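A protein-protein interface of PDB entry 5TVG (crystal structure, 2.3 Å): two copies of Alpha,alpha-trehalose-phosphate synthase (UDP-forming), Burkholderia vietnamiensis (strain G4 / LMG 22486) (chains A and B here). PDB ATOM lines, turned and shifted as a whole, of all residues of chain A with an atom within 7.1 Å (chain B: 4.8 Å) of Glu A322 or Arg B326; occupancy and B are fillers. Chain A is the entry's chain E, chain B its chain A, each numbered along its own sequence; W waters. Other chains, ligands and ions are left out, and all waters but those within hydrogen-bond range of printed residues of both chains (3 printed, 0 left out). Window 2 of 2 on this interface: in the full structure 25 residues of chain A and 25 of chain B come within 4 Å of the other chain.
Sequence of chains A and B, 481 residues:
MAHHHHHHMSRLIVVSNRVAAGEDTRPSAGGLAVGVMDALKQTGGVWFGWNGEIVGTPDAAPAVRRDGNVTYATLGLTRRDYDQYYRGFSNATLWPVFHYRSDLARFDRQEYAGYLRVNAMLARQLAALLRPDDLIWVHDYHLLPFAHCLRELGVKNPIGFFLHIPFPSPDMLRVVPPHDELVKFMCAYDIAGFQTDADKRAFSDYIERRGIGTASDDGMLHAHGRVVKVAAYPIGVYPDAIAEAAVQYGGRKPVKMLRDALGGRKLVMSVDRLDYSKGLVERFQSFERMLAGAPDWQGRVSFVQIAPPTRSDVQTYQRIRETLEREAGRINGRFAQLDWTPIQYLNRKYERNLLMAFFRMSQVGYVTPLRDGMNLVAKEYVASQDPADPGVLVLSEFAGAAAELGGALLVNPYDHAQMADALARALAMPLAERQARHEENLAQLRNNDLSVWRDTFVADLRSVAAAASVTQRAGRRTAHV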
ATOM      1  N   LEU A 274     -28.091  -1.349 -11.690  1.00  0.00           N
ATOM      2  CA  LEU A 274     -26.998  -0.738 -10.931  1.00  0.00           C
ATOM      3  C   LEU A 274     -25.718  -0.826 -11.768  1.00  0.00           C
ATOM      4  O   LEU A 274     -24.767  -1.543 -11.461  1.00  0.00           O
ATOM      5  CB  LEU A 274     -26.849  -1.413  -9.574  1.00  0.00           C
ATOM      6  CG  LEU A 274     -26.624  -0.475  -8.372  1.00  0.00           C
ATOM      7  CD1 LEU A 274     -26.529  -1.311  -7.078  1.00  0.00           C
ATOM      8  CD2 LEU A 274     -25.359   0.342  -8.571  1.00  0.00           C
ATOM      9  N   GLN A 315     -16.083  -7.360 -10.676  1.00  0.00           N
ATOM     10  CA  GLN A 315     -15.598  -6.558  -9.551  1.00  0.00           C
ATOM     11  C   GLN A 315     -15.908  -5.075  -9.736  1.00  0.00           C
ATOM     12  O   GLN A 315     -16.203  -4.378  -8.759  1.00  0.00           O
ATOM     13  CB  GLN A 315     -14.097  -6.772  -9.351  1.00  0.00           C
ATOM     14  N   TYR A 317     -18.489  -3.834 -10.991  1.00  0.00           N
ATOM     15  CA  TYR A 317     -19.880  -3.608 -10.593  1.00  0.00           C
ATOM     16  C   TYR A 317     -20.047  -3.638  -9.072  1.00  0.00           C
ATOM     17  O   TYR A 317     -20.932  -2.958  -8.526  1.00  0.00           O
ATOM     18  CB  TYR A 317     -20.806  -4.634 -11.257  1.00  0.00           C
ATOM     19  CG  TYR A 317     -21.113  -4.293 -12.700  1.00  0.00           C
ATOM     20  CD1 TYR A 317     -20.214  -4.591 -13.718  1.00  0.00           C
ATOM     21  CD2 TYR A 317     -22.288  -3.639 -13.037  1.00  0.00           C
ATOM     22  CE1 TYR A 317     -20.485  -4.265 -15.016  1.00  0.00           C
ATOM     23  CE2 TYR A 317     -22.571  -3.313 -14.345  1.00  0.00           C
ATOM     24  CZ  TYR A 317     -21.664  -3.615 -15.336  1.00  0.00           C
ATOM     25  OH  TYR A 317     -21.934  -3.281 -16.654  1.00  0.00           O
ATOM     26  N   GLN A 318     -19.200  -4.394  -8.376  1.00  0.00           N
ATOM     27  CA  GLN A 318     -19.255  -4.398  -6.921  1.00  0.00           C
ATOM     28  C   GLN A 318     -18.817  -3.053  -6.368  1.00  0.00           C
ATOM     29  O   GLN A 318     -19.416  -2.548  -5.407  1.00  0.00           O
ATOM     30  CB  GLN A 318     -18.394  -5.530  -6.365  1.00  0.00           C
ATOM     31  CG  GLN A 318     -18.783  -6.901  -6.895  1.00  0.00           C
ATOM     32  CD  GLN A 318     -17.684  -7.948  -6.740  1.00  0.00           C
ATOM     33  OE1 GLN A 318     -16.779  -7.816  -5.910  1.00  0.00           O
ATOM     34  NE2 GLN A 318     -17.766  -8.999  -7.541  1.00  0.00           N
ATOM     35  N   ARG A 319     -17.797  -2.443  -6.996  1.00  0.00           N
ATOM     36  CA  ARG A 319     -17.282  -1.158  -6.533  1.00  0.00           C
ATOM     37  C   ARG A 319     -18.316  -0.040  -6.695  1.00  0.00           C
ATOM     38  O   ARG A 319     -18.480   0.793  -5.795  1.00  0.00           O
ATOM     39  CB  ARG A 319     -15.974  -0.833  -7.257  1.00  0.00           C
ATOM     40  N   ILE A 320     -19.009   0.026  -7.833  1.00  0.00           N
ATOM     41  CA  ILE A 320     -19.991   1.103  -7.992  1.00  0.00           C
ATOM     42  C   ILE A 320     -21.155   0.905  -7.024  1.00  0.00           C
ATOM     43  O   ILE A 320     -21.735   1.885  -6.515  1.00  0.00           O
ATOM     44  CB  ILE A 320     -20.440   1.229  -9.475  1.00  0.00           C
ATOM     45  CG1 ILE A 320     -21.406   2.400  -9.679  1.00  0.00           C
ATOM     46  CG2 ILE A 320     -21.076  -0.034  -9.997  1.00  0.00           C
ATOM     47  CD1 ILE A 320     -20.841   3.748  -9.238  1.00  0.00           C
ATOM     48  N   ARG A 321     -21.501  -0.354  -6.732  1.00  0.00           N
ATOM     49  CA  ARG A 321     -22.558  -0.628  -5.766  1.00  0.00           C
ATOM     50  C   ARG A 321     -22.166  -0.153  -4.368  1.00  0.00           C
ATOM     51  O   ARG A 321     -22.954   0.509  -3.682  1.00  0.00           O
ATOM     52  CB  ARG A 321     -22.881  -2.123  -5.744  1.00  0.00           C
ATOM     53  CG  ARG A 321     -23.933  -2.517  -4.668  1.00  0.00           C
ATOM     54  CD  ARG A 321     -24.409  -3.966  -4.840  1.00  0.00           C
ATOM     55  NE  ARG A 321     -25.441  -4.282  -3.858  1.00  0.00           N
ATOM     56  CZ  ARG A 321     -26.059  -5.456  -3.749  1.00  0.00           C
ATOM     57  NH1 ARG A 321     -25.767  -6.456  -4.571  1.00  0.00           N
ATOM     58  NH2 ARG A 321     -26.978  -5.632  -2.807  1.00  0.00           N
ATOM     59  N   GLU A 322     -20.939  -0.473  -3.937  1.00  0.00           N
ATOM     60  CA  GLU A 322     -20.460  -0.017  -2.640  1.00  0.00           C
ATOM     61  C   GLU A 322     -20.467   1.493  -2.563  1.00  0.00           C
ATOM     62  O   GLU A 322     -20.889   2.073  -1.553  1.00  0.00           O
ATOM     63  CB  GLU A 322     -19.054  -0.550  -2.380  1.00  0.00           C
ATOM     64  CG  GLU A 322     -19.001  -2.061  -2.292  1.00  0.00           C
ATOM     65  CD  GLU A 322     -17.589  -2.616  -2.195  1.00  0.00           C
ATOM     66  OE1 GLU A 322     -17.421  -3.843  -2.391  1.00  0.00           O
ATOM     67  OE2 GLU A 322     -16.652  -1.838  -1.910  1.00  0.00           O
ATOM     68  N   THR A 323     -20.020   2.157  -3.628  1.00  0.00           N
ATOM     69  CA  THR A 323     -20.005   3.615  -3.612  1.00  0.00           C
ATOM     70  C   THR A 323     -21.418   4.161  -3.504  1.00  0.00           C
ATOM     71  O   THR A 323     -21.658   5.133  -2.784  1.00  0.00           O
ATOM     72  CB  THR A 323     -19.277   4.131  -4.862  1.00  0.00           C
ATOM     73  OG1 THR A 323     -17.960   3.582  -4.865  1.00  0.00           O
ATOM     74  CG2 THR A 323     -19.155   5.647  -4.857  1.00  0.00           C
ATOM     75  N   LEU A 324     -22.378   3.550  -4.214  1.00  0.00           N
ATOM     76  CA  LEU A 324     -23.751   4.062  -4.165  1.00  0.00           C
ATOM     77  C   LEU A 324     -24.395   3.840  -2.801  1.00  0.00           C
ATOM     78  O   LEU A 324     -25.159   4.694  -2.333  1.00  0.00           O
ATOM     79  CB  LEU A 324     -24.603   3.432  -5.267  1.00  0.00           C
ATOM     80  CG  LEU A 324     -26.002   4.040  -5.442  1.00  0.00           C
ATOM     81  CD1 LEU A 324     -25.865   5.509  -5.906  1.00  0.00           C
ATOM     82  CD2 LEU A 324     -26.852   3.225  -6.416  1.00  0.00           C
ATOM     83  N   GLU A 325     -24.157   2.673  -2.168  1.00  0.00           N
ATOM     84  CA  GLU A 325     -24.706   2.426  -0.826  1.00  0.00           C
ATOM     85  C   GLU A 325     -24.185   3.450   0.174  1.00  0.00           C
ATOM     86  O   GLU A 325     -24.917   3.891   1.077  1.00  0.00           O
ATOM     87  CB  GLU A 325     -24.360   0.999  -0.350  1.00  0.00           C
ATOM     88  CG  GLU A 325     -25.021  -0.074  -1.226  1.00  0.00           C
ATOM     89  CD  GLU A 325     -24.392  -1.439  -1.114  1.00  0.00           C
ATOM     90  OE1 GLU A 325     -23.242  -1.553  -0.641  1.00  0.00           O
ATOM     91  OE2 GLU A 325     -25.042  -2.419  -1.530  1.00  0.00           O
ATOM     92  N   ARG A 326     -22.897   3.789   0.076  1.00  0.00           N
ATOM     93  CA  ARG A 326     -22.337   4.772   1.004  1.00  0.00           C
ATOM     94  C   ARG A 326     -23.025   6.114   0.841  1.00  0.00           C
ATOM     95  O   ARG A 326     -23.404   6.756   1.830  1.00  0.00           O
ATOM     96  CB  ARG A 326     -20.840   4.918   0.761  1.00  0.00           C
ATOM     97  CG  ARG A 326     -20.091   5.677   1.826  1.00  0.00           C
ATOM     98  CD  ARG A 326     -20.023   7.130   1.403  1.00  0.00           C
ATOM     99  NE  ARG A 326     -19.486   8.025   2.424  1.00  0.00           N
ATOM    100  CZ  ARG A 326     -18.317   8.646   2.287  1.00  0.00           C
ATOM    101  NH1 ARG A 326     -17.569   8.413   1.200  1.00  0.00           N
ATOM    102  NH2 ARG A 326     -17.876   9.453   3.244  1.00  0.00           N
ATOM    103  N   GLU A 327     -23.234   6.530  -0.410  1.00  0.00           N
ATOM    104  CA  GLU A 327     -23.877   7.808  -0.688  1.00  0.00           C
ATOM    105  C   GLU A 327     -25.317   7.815  -0.209  1.00  0.00           C
ATOM    106  O   GLU A 327     -25.780   8.812   0.355  1.00  0.00           O
ATOM    107  CB  GLU A 327     -23.809   8.119  -2.194  1.00  0.00           C
ATOM    108  CG  GLU A 327     -22.412   8.542  -2.670  1.00  0.00           C
ATOM    109  CD  GLU A 327     -21.940   9.794  -1.959  1.00  0.00           C
ATOM    110  OE1 GLU A 327     -22.472  10.881  -2.236  1.00  0.00           O
ATOM    111  OE2 GLU A 327     -21.068   9.687  -1.071  1.00  0.00           O
ATOM    112  N   ALA A 328     -26.047   6.720  -0.416  1.00  0.00           N
ATOM    113  CA  ALA A 328     -27.395   6.655   0.140  1.00  0.00           C
ATOM    114  C   ALA A 328     -27.366   6.856   1.653  1.00  0.00           C
ATOM    115  O   ALA A 328     -28.124   7.663   2.196  1.00  0.00           O
ATOM    116  CB  ALA A 328     -28.045   5.307  -0.187  1.00  0.00           C
ATOM    117  N   GLY A 329     -26.487   6.128   2.348  1.00  0.00           N
ATOM    118  CA  GLY A 329     -26.415   6.257   3.802  1.00  0.00           C
ATOM    119  C   GLY A 329     -25.983   7.646   4.237  1.00  0.00           C
ATOM    120  O   GLY A 329     -26.564   8.228   5.160  1.00  0.00           O
ATOM    121  N   ARG A 330     -24.984   8.218   3.550  1.00  0.00           N
ATOM    122  CA  ARG A 330     -24.489   9.541   3.935  1.00  0.00           C
ATOM    123  C   ARG A 330     -25.566  10.600   3.741  1.00  0.00           C
ATOM    124  O   ARG A 330     -25.857  11.383   4.656  1.00  0.00           O
ATOM    125  CB  ARG A 330     -23.224   9.891   3.147  1.00  0.00           C
ATOM    126  CG  ARG A 330     -22.539  11.194   3.671  1.00  0.00           C
ATOM    127  CD  ARG A 330     -21.362  11.588   2.781  1.00  0.00           C
ATOM    128  NE  ARG A 330     -21.829  11.787   1.413  1.00  0.00           N
ATOM    129  CZ  ARG A 330     -22.574  12.826   1.030  1.00  0.00           C
ATOM    130  NH1 ARG A 330     -22.954  13.759   1.912  1.00  0.00           N
ATOM    131  NH2 ARG A 330     -22.974  12.914  -0.230  1.00  0.00           N
ATOM    132  N   TYR A 345     -33.968   3.852  -1.381  1.00  0.00           N
ATOM    133  CA  TYR A 345     -33.113   3.077  -2.263  1.00  0.00           C
ATOM    134  C   TYR A 345     -33.493   1.603  -2.116  1.00  0.00           C
ATOM    135  O   TYR A 345     -33.442   1.050  -1.008  1.00  0.00           O
ATOM    136  CB  TYR A 345     -31.645   3.343  -1.908  1.00  0.00           C
ATOM    137  CG  TYR A 345     -30.630   2.408  -2.556  1.00  0.00           C
ATOM    138  CD1 TYR A 345     -30.450   2.367  -3.947  1.00  0.00           C
ATOM    139  CD2 TYR A 345     -29.855   1.558  -1.768  1.00  0.00           C
ATOM    140  CE1 TYR A 345     -29.517   1.496  -4.520  1.00  0.00           C
ATOM    141  CE2 TYR A 345     -28.937   0.692  -2.327  1.00  0.00           C
ATOM    142  CZ  TYR A 345     -28.763   0.657  -3.695  1.00  0.00           C
ATOM    143  OH  TYR A 345     -27.836  -0.228  -4.222  1.00  0.00           O
ATOM    144  N   GLU B 322     -17.734   6.428   7.416  1.00  0.00           N
ATOM    145  CA  GLU B 322     -17.907   5.966   6.041  1.00  0.00           C
ATOM    146  C   GLU B 322     -18.366   4.517   6.005  1.00  0.00           C
ATOM    147  O   GLU B 322     -19.270   4.165   5.240  1.00  0.00           O
ATOM    148  CB  GLU B 322     -16.608   6.116   5.252  1.00  0.00           C
ATOM    149  CG  GLU B 322     -16.124   7.531   5.089  1.00  0.00           C
ATOM    150  CD  GLU B 322     -14.742   7.625   4.446  1.00  0.00           C
ATOM    151  OE1 GLU B 322     -14.278   6.619   3.861  1.00  0.00           O
ATOM    152  OE2 GLU B 322     -14.119   8.707   4.539  1.00  0.00           O
ATOM    153  N   THR B 323     -17.763   3.661   6.834  1.00  0.00           N
ATOM    154  CA  THR B 323     -18.170   2.257   6.862  1.00  0.00           C
ATOM    155  C   THR B 323     -19.629   2.115   7.271  1.00  0.00           C
ATOM    156  O   THR B 323     -20.370   1.333   6.668  1.00  0.00           O
ATOM    157  CB  THR B 323     -17.274   1.470   7.817  1.00  0.00           C
ATOM    158  OG1 THR B 323     -15.912   1.604   7.404  1.00  0.00           O
ATOM    159  CG2 THR B 323     -17.643  -0.005   7.807  1.00  0.00           C
ATOM    160  N   LEU B 324     -20.071   2.898   8.264  1.00  0.00           N
ATOM    161  CA  LEU B 324     -21.455   2.810   8.734  1.00  0.00           C
ATOM    162  C   LEU B 324     -22.430   3.304   7.678  1.00  0.00           C
ATOM    163  O   LEU B 324     -23.516   2.729   7.516  1.00  0.00           O
ATOM    164  CB  LEU B 324     -21.628   3.613  10.035  1.00  0.00           C
ATOM    165  CG  LEU B 324     -22.968   3.497  10.771  1.00  0.00           C
ATOM    166  CD1 LEU B 324     -23.237   2.040  11.325  1.00  0.00           C
ATOM    167  CD2 LEU B 324     -23.107   4.552  11.899  1.00  0.00           C
ATOM    168  N   GLU B 325     -22.077   4.388   6.970  1.00  0.00           N
ATOM    169  CA  GLU B 325     -22.948   4.879   5.905  1.00  0.00           C
ATOM    170  C   GLU B 325     -23.151   3.816   4.850  1.00  0.00           C
ATOM    171  O   GLU B 325     -24.275   3.596   4.388  1.00  0.00           O
ATOM    172  CB  GLU B 325     -22.388   6.165   5.266  1.00  0.00           C
ATOM    173  CG  GLU B 325     -22.415   7.347   6.259  1.00  0.00           C
ATOM    174  CD  GLU B 325     -21.578   8.541   5.825  1.00  0.00           C
ATOM    175  OE1 GLU B 325     -20.698   8.394   4.958  1.00  0.00           O
ATOM    176  OE2 GLU B 325     -21.809   9.634   6.372  1.00  0.00           O
ATOM    177  N   ARG B 326     -22.079   3.132   4.476  1.00  0.00           N
ATOM    178  CA  ARG B 326     -22.198   2.071   3.489  1.00  0.00           C
ATOM    179  C   ARG B 326     -23.115   0.963   4.003  1.00  0.00           C
ATOM    180  O   ARG B 326     -23.998   0.502   3.280  1.00  0.00           O
ATOM    181  CB  ARG B 326     -20.803   1.557   3.129  1.00  0.00           C
ATOM    182  CG  ARG B 326     -20.738   0.688   1.916  1.00  0.00           C
ATOM    183  CD  ARG B 326     -20.716  -0.762   2.348  1.00  0.00           C
ATOM    184  NE  ARG B 326     -20.870  -1.685   1.231  1.00  0.00           N
ATOM    185  CZ  ARG B 326     -20.501  -2.952   1.290  1.00  0.00           C
ATOM    186  NH1 ARG B 326     -20.669  -3.748   0.241  1.00  0.00           N
ATOM    187  NH2 ARG B 326     -19.945  -3.407   2.406  1.00  0.00           N
ATOM    188  N   GLU B 327     -22.986   0.593   5.285  1.00  0.00           N
ATOM    189  CA  GLU B 327     -23.846  -0.448   5.831  1.00  0.00           C
ATOM    190  C   GLU B 327     -25.311  -0.019   5.875  1.00  0.00           C
ATOM    191  O   GLU B 327     -26.197  -0.807   5.507  1.00  0.00           O
ATOM    192  CB  GLU B 327     -23.353  -0.847   7.230  1.00  0.00           C
ATOM    193  CG  GLU B 327     -22.050  -1.641   7.155  1.00  0.00           C
ATOM    194  CD  GLU B 327     -22.215  -2.931   6.375  1.00  0.00           C
ATOM    195  OE1 GLU B 327     -22.872  -3.853   6.882  1.00  0.00           O
ATOM    196  OE2 GLU B 327     -21.726  -3.020   5.225  1.00  0.00           O
ATOM    197  N   ALA B 328     -25.597   1.226   6.275  1.00  0.00           N
ATOM    198  CA  ALA B 328     -26.987   1.685   6.253  1.00  0.00           C
ATOM    199  C   ALA B 328     -27.565   1.584   4.847  1.00  0.00           C
ATOM    200  O   ALA B 328     -28.674   1.068   4.644  1.00  0.00           O
ATOM    201  CB  ALA B 328     -27.095   3.123   6.752  1.00  0.00           C
ATOM    202  N   GLY B 329     -26.819   2.057   3.857  1.00  0.00           N
ATOM    203  CA  GLY B 329     -27.330   1.995   2.499  1.00  0.00           C
ATOM    204  C   GLY B 329     -27.540   0.571   2.033  1.00  0.00           C
ATOM    205  O   GLY B 329     -28.582   0.247   1.460  1.00  0.00           O
ATOM    206  N   ARG B 330     -26.570  -0.307   2.300  1.00  0.00           N
ATOM    207  CA  ARG B 330     -26.671  -1.691   1.828  1.00  0.00           C
ATOM    208  C   ARG B 330     -27.825  -2.419   2.503  1.00  0.00           C
ATOM    209  O   ARG B 330     -28.615  -3.095   1.837  1.00  0.00           O
ATOM    210  CB  ARG B 330     -25.352  -2.434   2.069  1.00  0.00           C
ATOM    211  CG  ARG B 330     -25.313  -3.855   1.471  1.00  0.00           C
ATOM    212  CD  ARG B 330     -24.051  -4.594   1.894  1.00  0.00           C
ATOM    213  NE  ARG B 330     -23.958  -4.681   3.366  1.00  0.00           N
ATOM    214  CZ  ARG B 330     -24.718  -5.480   4.128  1.00  0.00           C
ATOM    215  NH1 ARG B 330     -25.642  -6.265   3.578  1.00  0.00           N
ATOM    216  NH2 ARG B 330     -24.558  -5.488   5.448  1.00  0.00           N
HETATM  217  O   HOH W   1     -22.818  -4.155  -1.389  1.00  0.00           O
HETATM  218  O   HOH W   2     -19.334  10.956   5.620  1.00  0.00           O
HETATM  219  O   HOH W   3     -28.040  -3.845  -0.870  1.00  0.00           O
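The backbone carbonyl oxygen (O) of Glu A325 sits close to the backbone carbonyl oxygen (O) of Glu B325. OE1 of Glu B325 is in salt-bridge range of NE of Arg A326, 2.8 Å away. OE1 of Glu A325 lies within salt-bridge range of NE of Arg B326 (3.0 Å).
The guanidinium group (NH2) of Arg A330 is in salt-bridge range of the side-chain carboxylate (OE1) of Glu A327 (2.9 Å). NE of Arg A321 is in salt-bridge range of OE2 of Glu A325 (3.0 Å). OE1 of Glu B327 lies within salt-bridge range of NH2 of Arg B330, at 2.8 Å. NH2 of Arg B326 lies within salt-bridge range of OE2 of Glu B327.
Among the printed residues, merely in contact across the chains: Glu A322 with Arg B326 (3.5 Å), Glu A325 with Gly B329 (3.4 Å), Glu A325 with Arg B330 (3.3 Å), Arg A326 with Glu B322 (3.2 Å), Arg A326 with Arg B326 (3.7 Å), Gly A329 with Glu B325 (3.5 Å), Arg A330 with Glu B325 (3.2 Å) and Tyr A345 with Gly B329 (3.7 Å).
Glu A322 touches one residue of chain B. Of chain A, only Glu A322 (3.5 Å), Glu A325 (3.0 Å) and Arg A326 (3.7 Å) come within 4 Å of Arg B326. Of the printed residues of chain B, Tyr A345 touches Gly B329 (3.7 Å). Printed residues of chain A within 4 Å of Glu B322: Arg A326. The nearest printed residue of chain B that does not touch Glu A322 is Glu B325 (7.0 Å). The nearest residue of chain A that does not touch Arg B326 is Gly A329 (5.4 Å).
Of the 17 printed residues of chain A, 6 touch a printed residue of chain B. Of the 9 printed residues of chain B, 5 touch a printed residue of chain A. Printed residues of chain B that touch a printed residue of chain A: Glu B322, Glu B325, Arg B326, Gly B329 and Arg B330. Among the printed residues, 11 pairs touch across the chains. Among the printed residues, Asp or Glu carboxylates within 4 Å of a Lys or Arg side-chain nitrogen of the other chain: Glu A325 with Arg B326 (3.0 Å) and Arg A326 with Glu B325 (2.8 Å).
Glu A322 touches Arg B326, and with the chains exchanged Arg A326 touches Glu B322. Glu B325 touches its own counterpart, Glu A325. Glu A325 touches Arg B330, and with the chains exchanged Arg A330 touches Glu B325. Arg A326 touches its own counterpart, Arg B326. 9 positions are printed for both chains. Of the 11 pairs that touch across the chains among the printed residues, 10 have their exchanged pair printed and touching as well.
Water W1 lies within hydrogen-bond range of the guanidinium group of Arg B326 (2.7 Å) and the side-chain carboxylate of Glu A325 (2.7 Å). Water W3 lies within hydrogen-bond range of the guanidinium group of Arg A321 (2.8 Å), the backbone carbonyl oxygen of Arg B330 (2.9 Å) and the side-chain carboxylate of Glu A325 (3.4 Å). Water W2 bridges OE2 of Glu B325 (2.9 Å) and NH2 of Arg A326 (3.2 Å).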
